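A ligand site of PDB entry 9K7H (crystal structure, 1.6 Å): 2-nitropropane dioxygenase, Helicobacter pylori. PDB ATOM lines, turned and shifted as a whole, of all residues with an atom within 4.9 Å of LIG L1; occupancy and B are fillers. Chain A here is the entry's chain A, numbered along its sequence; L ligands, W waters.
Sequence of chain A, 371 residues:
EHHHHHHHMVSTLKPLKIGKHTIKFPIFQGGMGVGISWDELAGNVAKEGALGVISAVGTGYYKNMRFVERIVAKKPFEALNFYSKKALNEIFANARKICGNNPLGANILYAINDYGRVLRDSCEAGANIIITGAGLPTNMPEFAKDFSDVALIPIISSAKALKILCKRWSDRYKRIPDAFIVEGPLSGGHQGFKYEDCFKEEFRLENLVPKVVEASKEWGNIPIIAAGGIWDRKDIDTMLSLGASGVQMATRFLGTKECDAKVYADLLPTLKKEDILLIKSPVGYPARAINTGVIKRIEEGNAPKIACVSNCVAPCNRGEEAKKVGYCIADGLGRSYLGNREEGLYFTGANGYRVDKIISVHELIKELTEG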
ATOM      1  N   GLY A  30       9.332   6.046  -9.296  1.00  0.00           N
ATOM      2  CA  GLY A  30      10.037   5.195  -8.345  1.00  0.00           C
ATOM      3  C   GLY A  30       9.097   4.217  -7.647  1.00  0.00           C
ATOM      4  O   GLY A  30       7.961   4.546  -7.291  1.00  0.00           O
ATOM      5  N   GLY A  31       9.569   2.990  -7.462  1.00  0.00           N
ATOM      6  CA  GLY A  31       8.743   1.976  -6.816  1.00  0.00           C
ATOM      7  C   GLY A  31       8.466   2.333  -5.371  1.00  0.00           C
ATOM      8  O   GLY A  31       9.336   2.863  -4.663  1.00  0.00           O
ATOM      9  N   MET A  32       7.246   2.052  -4.915  1.00  0.00           N
ATOM     10  CA  MET A  32       6.847   2.465  -3.576  1.00  0.00           C
ATOM     11  C   MET A  32       5.997   1.364  -2.932  1.00  0.00           C
ATOM     12  O   MET A  32       4.913   1.052  -3.432  1.00  0.00           O
ATOM     13  CB  MET A  32       6.045   3.771  -3.678  1.00  0.00           C
ATOM     14  CG  MET A  32       6.918   4.979  -3.944  1.00  0.00           C
ATOM     15  SD  MET A  32       6.013   6.543  -3.988  1.00  0.00           S
ATOM     16  CE  MET A  32       5.536   6.566  -5.709  1.00  0.00           C
ATOM     17  N   GLY A  33       6.471   0.791  -1.813  1.00  0.00           N
ATOM     18  CA  GLY A  33       5.721  -0.175  -1.071  1.00  0.00           C
ATOM     19  C   GLY A  33       5.282   0.405   0.265  1.00  0.00           C
ATOM     20  O   GLY A  33       5.751   1.455   0.701  1.00  0.00           O
ATOM     21  N   ILE A  36       1.714   1.001  -2.797  1.00  0.00           N
ATOM     22  CA  ILE A  36       1.548   2.336  -3.324  1.00  0.00           C
ATOM     23  C   ILE A  36       1.654   2.326  -4.833  1.00  0.00           C
ATOM     24  O   ILE A  36       0.773   2.854  -5.527  1.00  0.00           O
ATOM     25  CB  ILE A  36       2.545   3.310  -2.681  1.00  0.00           C
ATOM     26  CG1 ILE A  36       2.120   3.554  -1.224  1.00  0.00           C
ATOM     27  CG2 ILE A  36       2.626   4.583  -3.527  1.00  0.00           C
ATOM     28  CD1 ILE A  36       3.172   3.427  -0.216  1.00  0.00           C
ATOM     29  N   SER A  55       5.947  -2.153  -7.227  1.00  0.00           N
ATOM     30  CA  SER A  55       6.648  -2.567  -6.016  1.00  0.00           C
ATOM     31  C   SER A  55       6.324  -4.013  -5.706  1.00  0.00           C
ATOM     32  O   SER A  55       5.156  -4.387  -5.634  1.00  0.00           O
ATOM     33  CB  SER A  55       6.238  -1.668  -4.843  1.00  0.00           C
ATOM     34  OG  SER A  55       6.803  -2.156  -3.629  1.00  0.00           O
ATOM     35  N   VAL A  57       7.149  -5.745  -2.976  1.00  0.00           N
ATOM     36  CA  VAL A  57       7.240  -6.051  -1.551  1.00  0.00           C
ATOM     37  C   VAL A  57       5.843  -6.043  -0.947  1.00  0.00           C
ATOM     38  O   VAL A  57       5.033  -5.146  -1.213  1.00  0.00           O
ATOM     39  CB  VAL A  57       8.193  -5.090  -0.815  1.00  0.00           C
ATOM     40  CG1 VAL A  57       9.571  -5.071  -1.506  1.00  0.00           C
ATOM     41  CG2 VAL A  57       7.610  -3.682  -0.666  1.00  0.00           C
ATOM     42  N   ASN A 107      10.389  -3.190  -8.459  1.00  0.00           N
ATOM     43  CA  ASN A 107      11.339  -2.770  -7.439  1.00  0.00           C
ATOM     44  C   ASN A 107      11.375  -3.804  -6.324  1.00  0.00           C
ATOM     45  O   ASN A 107      10.337  -4.176  -5.782  1.00  0.00           O
ATOM     46  CB  ASN A 107      10.943  -1.385  -6.901  1.00  0.00           C
ATOM     47  CG  ASN A 107      11.850  -0.903  -5.800  1.00  0.00           C
ATOM     48  OD1 ASN A 107      11.928  -1.524  -4.730  1.00  0.00           O
ATOM     49  ND2 ASN A 107      12.529   0.221  -6.031  1.00  0.00           N
ATOM     50  N   LEU A 109      13.645  -4.681  -2.751  1.00  0.00           N
ATOM     51  CA  LEU A 109      14.706  -4.318  -1.818  1.00  0.00           C
ATOM     52  C   LEU A 109      15.638  -5.501  -1.599  1.00  0.00           C
ATOM     53  O   LEU A 109      15.191  -6.643  -1.435  1.00  0.00           O
ATOM     54  CB  LEU A 109      14.134  -3.899  -0.450  1.00  0.00           C
ATOM     55  CG  LEU A 109      13.692  -2.430  -0.307  1.00  0.00           C
ATOM     56  CD1 LEU A 109      12.719  -2.078  -1.392  1.00  0.00           C
ATOM     57  CD2 LEU A 109      13.101  -2.144   1.062  1.00  0.00           C
ATOM     58  N   ILE A 155      20.398   0.438  -7.306  1.00  0.00           N
ATOM     59  CA  ILE A 155      20.403   1.772  -6.723  1.00  0.00           C
ATOM     60  C   ILE A 155      21.670   1.933  -5.905  1.00  0.00           C
ATOM     61  O   ILE A 155      21.948   1.099  -5.026  1.00  0.00           O
ATOM     62  CB  ILE A 155      19.165   2.024  -5.845  1.00  0.00           C
ATOM     63  CG1 ILE A 155      17.874   1.863  -6.664  1.00  0.00           C
ATOM     64  CG2 ILE A 155      19.235   3.408  -5.271  1.00  0.00           C
ATOM     65  CD1 ILE A 155      16.595   1.948  -5.803  1.00  0.00           C
ATOM     66  N   GLU A 183      21.237   7.810  -5.823  1.00  0.00           N
ATOM     67  CA  GLU A 183      20.497   8.546  -4.809  1.00  0.00           C
ATOM     68  C   GLU A 183      21.459   8.866  -3.677  1.00  0.00           C
ATOM     69  O   GLU A 183      22.350   8.067  -3.375  1.00  0.00           O
ATOM     70  CB  GLU A 183      19.319   7.723  -4.273  1.00  0.00           C
ATOM     71  CG  GLU A 183      19.707   6.676  -3.251  1.00  0.00           C
ATOM     72  CD  GLU A 183      18.524   5.888  -2.708  1.00  0.00           C
ATOM     73  OE1 GLU A 183      17.388   6.424  -2.727  1.00  0.00           O
ATOM     74  OE2 GLU A 183      18.732   4.750  -2.237  1.00  0.00           O
ATOM     75  N   GLY A 228      15.932  11.427  -6.092  1.00  0.00           N
ATOM     76  CA  GLY A 228      15.819  12.081  -4.804  1.00  0.00           C
ATOM     77  C   GLY A 228      15.657  13.586  -4.870  1.00  0.00           C
ATOM     78  O   GLY A 228      16.600  14.301  -5.237  1.00  0.00           O
ATOM     79  N   GLY A 229      14.476  14.105  -4.523  1.00  0.00           N
ATOM     80  CA  GLY A 229      14.277  15.541  -4.486  1.00  0.00           C
ATOM     81  C   GLY A 229      14.003  16.181  -5.810  1.00  0.00           C
ATOM     82  O   GLY A 229      13.981  17.414  -5.897  1.00  0.00           O
ATOM     83  N   ILE A 230      13.787  15.394  -6.860  1.00  0.00           N
ATOM     84  CA  ILE A 230      13.465  15.912  -8.181  1.00  0.00           C
ATOM     85  C   ILE A 230      11.960  16.143  -8.221  1.00  0.00           C
ATOM     86  O   ILE A 230      11.164  15.215  -8.034  1.00  0.00           O
ATOM     87  CB  ILE A 230      13.917  14.934  -9.274  1.00  0.00           C
ATOM     88  CG1 ILE A 230      15.442  14.762  -9.168  1.00  0.00           C
ATOM     89  CG2 ILE A 230      13.529  15.424 -10.637  1.00  0.00           C
ATOM     90  CD1 ILE A 230      15.981  13.583  -9.954  1.00  0.00           C
ATOM     91  N   GLN A 248      14.518   9.500 -11.646  1.00  0.00           N
ATOM     92  CA  GLN A 248      13.511   8.720 -10.935  1.00  0.00           C
ATOM     93  C   GLN A 248      12.832   9.636  -9.921  1.00  0.00           C
ATOM     94  O   GLN A 248      13.501  10.356  -9.178  1.00  0.00           O
ATOM     95  CB  GLN A 248      14.122   7.525 -10.213  1.00  0.00           C
ATOM     96  CG  GLN A 248      13.053   6.740  -9.455  1.00  0.00           C
ATOM     97  CD  GLN A 248      13.600   5.515  -8.766  1.00  0.00           C
ATOM     98  OE1 GLN A 248      13.599   4.427  -9.325  1.00  0.00           O
ATOM     99  NE2 GLN A 248      14.004   5.683  -7.511  1.00  0.00           N
ATOM    100  N   MET A 249      11.501   9.574  -9.889  1.00  0.00           N
ATOM    101  CA  MET A 249      10.671  10.448  -9.058  1.00  0.00           C
ATOM    102  C   MET A 249       9.660   9.574  -8.326  1.00  0.00           C
ATOM    103  O   MET A 249       8.974   8.767  -8.954  1.00  0.00           O
ATOM    104  CB  MET A 249       9.971  11.493  -9.939  1.00  0.00           C
ATOM    105  CG  MET A 249      10.965  12.439 -10.621  1.00  0.00           C
ATOM    106  SD  MET A 249      10.235  13.541 -11.864  1.00  0.00           S
ATOM    107  CE  MET A 249       9.097  14.520 -10.901  1.00  0.00           C
ATOM    108  N   ALA A 250       9.571   9.735  -7.010  1.00  0.00           N
ATOM    109  CA  ALA A 250       8.582   8.983  -6.236  1.00  0.00           C
ATOM    110  C   ALA A 250       7.507   9.905  -5.690  1.00  0.00           C
ATOM    111  O   ALA A 250       6.328   9.731  -6.011  1.00  0.00           O
ATOM    112  CB  ALA A 250       9.241   8.186  -5.106  1.00  0.00           C
ATOM    113  N   THR A 251       7.887  10.881  -4.856  1.00  0.00           N
ATOM    114  CA  THR A 251       6.897  11.677  -4.145  1.00  0.00           C
ATOM    115  C   THR A 251       5.909  12.350  -5.090  1.00  0.00           C
ATOM    116  O   THR A 251       4.718  12.409  -4.794  1.00  0.00           O
ATOM    117  CB  THR A 251       7.596  12.721  -3.270  1.00  0.00           C
ATOM    118  OG1 THR A 251       8.328  12.044  -2.240  1.00  0.00           O
ATOM    119  CG2 THR A 251       6.590  13.662  -2.618  1.00  0.00           C
ATOM    120  N   LEU A 254       3.419   9.793  -5.808  1.00  0.00           N
ATOM    121  CA  LEU A 254       2.661   9.528  -4.592  1.00  0.00           C
ATOM    122  C   LEU A 254       1.464  10.448  -4.475  1.00  0.00           C
ATOM    123  O   LEU A 254       0.418  10.057  -3.933  1.00  0.00           O
ATOM    124  CB  LEU A 254       3.595   9.690  -3.384  1.00  0.00           C
ATOM    125  CG  LEU A 254       3.037   9.317  -2.003  1.00  0.00           C
ATOM    126  CD1 LEU A 254       2.574   7.867  -1.931  1.00  0.00           C
ATOM    127  CD2 LEU A 254       4.067   9.620  -0.935  1.00  0.00           C
ATOM    128  N   TYR A 264      -3.184   8.254   0.814  1.00  0.00           N
ATOM    129  CA  TYR A 264      -2.283   9.376   0.556  1.00  0.00           C
ATOM    130  C   TYR A 264      -2.983  10.576  -0.062  1.00  0.00           C
ATOM    131  O   TYR A 264      -2.614  11.716   0.210  1.00  0.00           O
ATOM    132  CB  TYR A 264      -1.087   8.925  -0.290  1.00  0.00           C
ATOM    133  CG  TYR A 264      -0.052   8.145   0.523  1.00  0.00           C
ATOM    134  CD1 TYR A 264       0.922   8.829   1.243  1.00  0.00           C
ATOM    135  CD2 TYR A 264      -0.102   6.747   0.649  1.00  0.00           C
ATOM    136  CE1 TYR A 264       1.863   8.149   2.021  1.00  0.00           C
ATOM    137  CE2 TYR A 264       0.841   6.056   1.414  1.00  0.00           C
ATOM    138  CZ  TYR A 264       1.831   6.765   2.098  1.00  0.00           C
ATOM    139  OH  TYR A 264       2.763   6.111   2.884  1.00  0.00           O
ATOM    140  N   PHE A 347       5.045   6.888   4.592  1.00  0.00           N
ATOM    141  CA  PHE A 347       6.325   7.393   4.121  1.00  0.00           C
ATOM    142  C   PHE A 347       6.140   8.586   3.178  1.00  0.00           C
ATOM    143  O   PHE A 347       5.083   8.766   2.562  1.00  0.00           O
ATOM    144  CB  PHE A 347       7.111   6.300   3.386  1.00  0.00           C
ATOM    145  CG  PHE A 347       7.735   5.243   4.265  1.00  0.00           C
ATOM    146  CD1 PHE A 347       7.840   5.414   5.633  1.00  0.00           C
ATOM    147  CD2 PHE A 347       8.204   4.066   3.704  1.00  0.00           C
ATOM    148  CE1 PHE A 347       8.435   4.421   6.423  1.00  0.00           C
ATOM    149  CE2 PHE A 347       8.795   3.073   4.485  1.00  0.00           C
ATOM    150  CZ  PHE A 347       8.912   3.250   5.849  1.00  0.00           C
ATOM    151  N   THR A 348       7.192   9.393   3.064  1.00  0.00           N
ATOM    152  CA  THR A 348       7.220  10.491   2.106  1.00  0.00           C
ATOM    153  C   THR A 348       8.674  10.865   1.817  1.00  0.00           C
ATOM    154  O   THR A 348       9.542  10.765   2.687  1.00  0.00           O
ATOM    155  CB  THR A 348       6.445  11.703   2.613  1.00  0.00           C
ATOM    156  OG1 THR A 348       6.460  12.740   1.630  1.00  0.00           O
ATOM    157  CG2 THR A 348       7.043  12.226   3.947  1.00  0.00           C
ATOM    158  N   GLY A 349       8.916  11.334   0.604  1.00  0.00           N
ATOM    159  CA  GLY A 349      10.145  12.046   0.348  1.00  0.00           C
ATOM    160  C   GLY A 349      10.146  13.396   1.054  1.00  0.00           C
ATOM    161  O   GLY A 349       9.152  13.856   1.599  1.00  0.00           O
ATOM    162  N   ALA A 350      11.308  14.064   1.016  1.00  0.00           N
ATOM    163  CA  ALA A 350      11.422  15.335   1.708  1.00  0.00           C
ATOM    164  C   ALA A 350      10.472  16.400   1.152  1.00  0.00           C
ATOM    165  O   ALA A 350      10.057  17.301   1.891  1.00  0.00           O
ATOM    166  CB  ALA A 350      12.866  15.837   1.660  1.00  0.00           C
HETATM  167  N1  LIG L   1      12.350   2.908  -2.523  1.00  0.00           N
HETATM  168  C1  LIG L   1      12.586   1.621  -2.959  1.00  0.00           C
HETATM  169  O1  LIG L   1      13.636   1.321  -3.547  1.00  0.00           O
HETATM  170  N2  LIG L   1      11.619   0.644  -2.718  1.00  0.00           N
HETATM  171  C2  LIG L   1      10.433   0.913  -2.066  1.00  0.00           C
HETATM  172  O2  LIG L   1       9.639  -0.017  -1.924  1.00  0.00           O
HETATM  173  C3  LIG L   1      10.192   2.202  -1.618  1.00  0.00           C
HETATM  174  N3  LIG L   1       9.034   2.525  -0.980  1.00  0.00           N
HETATM  175  C4  LIG L   1       8.745   3.839  -0.803  1.00  0.00           C
HETATM  176  C5  LIG L   1       7.469   4.226  -0.370  1.00  0.00           C
HETATM  177  C6  LIG L   1       7.134   5.567  -0.213  1.00  0.00           C
HETATM  178  C7  LIG L   1       5.843   5.959   0.183  1.00  0.00           C
HETATM  179  C8  LIG L   1       8.092   6.537  -0.494  1.00  0.00           C
HETATM  180  C9  LIG L   1       7.785   7.899  -0.347  1.00  0.00           C
HETATM  181  C10 LIG L   1       9.343   6.150  -0.906  1.00  0.00           C
HETATM  182  C11 LIG L   1       9.702   4.809  -1.062  1.00  0.00           C
HETATM  183  N4  LIG L   1      10.944   4.457  -1.498  1.00  0.00           N
HETATM  184  C12 LIG L   1      11.156   3.192  -1.855  1.00  0.00           C
HETATM  185  C13 LIG L   1      11.981   5.447  -1.875  1.00  0.00           C
HETATM  186  C14 LIG L   1      11.600   6.009  -3.286  1.00  0.00           C
HETATM  187  O3  LIG L   1      11.637   5.014  -4.318  1.00  0.00           O
HETATM  188  C15 LIG L   1      12.558   7.059  -3.785  1.00  0.00           C
HETATM  189  O4  LIG L   1      13.877   6.513  -3.866  1.00  0.00           O
HETATM  190  C16 LIG L   1      12.553   8.380  -3.014  1.00  0.00           C
HETATM  191  O5  LIG L   1      11.354   8.604  -2.254  1.00  0.00           O
HETATM  192  C17 LIG L   1      12.503   9.245  -4.235  1.00  0.00           C
HETATM  193  O6  LIG L   1      12.758  10.570  -3.966  1.00  0.00           O
HETATM  194  P1  LIG L   1      11.586  11.548  -4.169  1.00  0.00           P
HETATM  195  O7  LIG L   1      11.358  11.639  -5.623  1.00  0.00           O
HETATM  196  O8  LIG L   1      10.438  10.987  -3.422  1.00  0.00           O
HETATM  197  O9  LIG L   1      12.261  12.713  -3.572  1.00  0.00           O
HETATM  198  C1  LG2 L   2      12.987   2.027   3.182  1.00  0.00           C
HETATM  199  C2  LG2 L   2      14.136   2.121   5.252  1.00  0.00           C
HETATM  200  C3  LG2 L   2      10.616  -0.952   3.053  1.00  0.00           C
HETATM  201  C4  LG2 L   2      11.130  -1.923   3.902  1.00  0.00           C
HETATM  202  C5  LG2 L   2      10.416  -3.099   4.128  1.00  0.00           C
HETATM  203  C6  LG2 L   2       9.409  -1.165   2.432  1.00  0.00           C
HETATM  204  C7  LG2 L   2      12.676   5.411   1.709  1.00  0.00           C
HETATM  205  C8  LG2 L   2      11.445   5.440   2.346  1.00  0.00           C
HETATM  206  C9  LG2 L   2      10.868   6.666   2.663  1.00  0.00           C
HETATM  207  C10 LG2 L   2      11.495   7.851   2.321  1.00  0.00           C
HETATM  208  C11 LG2 L   2      12.719   7.814   1.675  1.00  0.00           C
HETATM  209  C12 LG2 L   2      13.438   9.091   1.275  1.00  0.00           C
HETATM  210  C13 LG2 L   2      13.295   6.600   1.371  1.00  0.00           C
HETATM  211  C14 LG2 L   2      13.931   2.649   3.992  1.00  0.00           C
HETATM  212  C15 LG2 L   2      13.401   1.023   5.663  1.00  0.00           C
HETATM  213  C16 LG2 L   2      12.294   0.923   3.639  1.00  0.00           C
HETATM  214  C17 LG2 L   2       9.196  -3.274   3.496  1.00  0.00           C
HETATM  215  C18 LG2 L   2       8.699  -2.320   2.649  1.00  0.00           C
HETATM  216  N1  LG2 L   2      13.385   4.196   1.339  1.00  0.00           N
HETATM  217  N2  LG2 L   2      12.519   0.473   4.847  1.00  0.00           N
HETATM  218  N3  LG2 L   2      11.316   0.292   2.765  1.00  0.00           N
HETATM  219  O1  LG2 L   2      13.207   1.645   0.567  1.00  0.00           O
HETATM  220  O2  LG2 L   2      12.961  10.212   1.569  1.00  0.00           O
HETATM  221  O3  LG2 L   2      14.504   9.030   0.615  1.00  0.00           O
HETATM  222  O4  LG2 L   2      11.247   2.696   1.226  1.00  0.00           O
HETATM  223  S1  LG2 L   2      12.682   2.649   1.508  1.00  0.00           S
HETATM  224 CL1  LG2 L   2       8.237  -4.738   3.751  1.00  0.00          CL
HETATM  225 CL2  LG2 L   2       8.745   0.065   1.344  1.00  0.00          CL
HETATM  226  O   HOH W   1      11.773  14.508  -1.692  1.00  0.00           O
HETATM  227  O   HOH W   2       9.366  -2.350  -3.379  1.00  0.00           O
HETATM  228  O   HOH W   3      15.966   1.586  -1.770  1.00  0.00           O
HETATM  229  O   HOH W   4       9.348  13.337  -6.794  1.00  0.00           O
HETATM  230  O   HOH W   5      13.437  12.309  -7.112  1.00  0.00           O
HETATM  231  O   HOH W   6      14.817  -1.123  -3.832  1.00  0.00           O
HETATM  232  O   HOH W   7      13.365   8.813  -6.873  1.00  0.00           O
HETATM  233  O   HOH W   8      11.049  15.361  -4.896  1.00  0.00           O
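OG1 of Thr 251 is in hydrogen-bond range of N of Gly 349 (3.0 Å).
The backbone NH (N) of Gly 33 lies close to the side-chain hydroxyl (OG) of Ser 55 (3.5 Å).
The backbone NH of Phe 347 sits at hydrogen-bond distance from the side-chain hydroxyl of Tyr 264, 3.0 Å away.
The backbone carbonyl oxygen (O) of Met 249 sits at hydrogen-bond distance from the backbone NH (N) of Gly 30 (2.8 Å).
N of Thr 251 is in hydrogen-bond range of O8 of LIG L1 (2.9 Å).
An oxygen (O8) of LIG L1 sits at hydrogen-bond distance from the side-chain hydroxyl of Thr 251.
The backbone NH (N) of Gly 229 lies within hydrogen-bond range of an oxygen (O9) of LIG L1, at 2.8 Å.
ND2 of Asn 107 sits at hydrogen-bond distance from O1 of LIG L1, at 2.9 Å.
N of Ala 250 lies within hydrogen-bond range of O7 of LIG L1, at 3.0 Å.
O of Gly 31 sits at hydrogen-bond distance from O3 of LIG L1.
The backbone NH of Gly 33 is in hydrogen-bond range of a nitrogen (N3) of LIG L1.
CA of Met 32 touches N3 of LIG L1, at 3.4 Å.
CD1 of Ile 36 touches C7 of LIG L1, 3.7 Å away.
OG of Ser 55 touches O2 of LIG L1 (3.9 Å).
CD1 of Leu 109 touches N2 of LIG L1, 3.2 Å away.
CD1 of Ile 155 touches O1 of LIG L1, at 3.8 Å.
Glu 183 touches LIG L1.
Gly 228 touches LIG L1 (CA to O6, 3.5 Å).
Gln 248 touches LIG L1.
Met 249 touches LIG L1.
Phe 347 touches LIG L1 (CB to C7, 3.5 Å).
Thr 348 touches LIG L1.
Gly 349 touches LIG L1 (N to C9, 3.7 Å).
Hydrophobic or aromatic side chains that line LIG L1: Met 32, Ile 36, Leu 109, Ile 155, Ala 250 and Phe 347.
Water W1 bridges an oxygen (O9) of LIG L1 (2.6 Å) and the backbone NH of Ala 350 (2.8 Å).
Water W6 lies within hydrogen-bond range of an oxygen (O1) of LIG L1 (2.7 Å) and the side-chain amide oxygen (OD1) of Asn 107 (3.1 Å).
Water W2 lies within hydrogen-bond range of the side-chain hydroxyl of Ser 55 (2.6 Å), an oxygen (O2) of LIG L1 (2.8 Å) and the side-chain amide oxygen of Asn 107 (3.0 Å).
Water W7 bridges O of Gln 248 (2.8 Å) and O6 of LIG L1 (3.5 Å).
Water W4 lies within hydrogen-bond range of an oxygen (O7) of LIG L1 (2.9 Å), the backbone carbonyl oxygen (O) of Ile 230 (2.9 Å) and the backbone NH (N) of Thr 251 (3.5 Å).
Water W8 lies within hydrogen-bond range of the backbone carbonyl oxygen (O) of Ile 230 (3.1 Å) and an oxygen (O9) of LIG L1 (3.2 Å).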
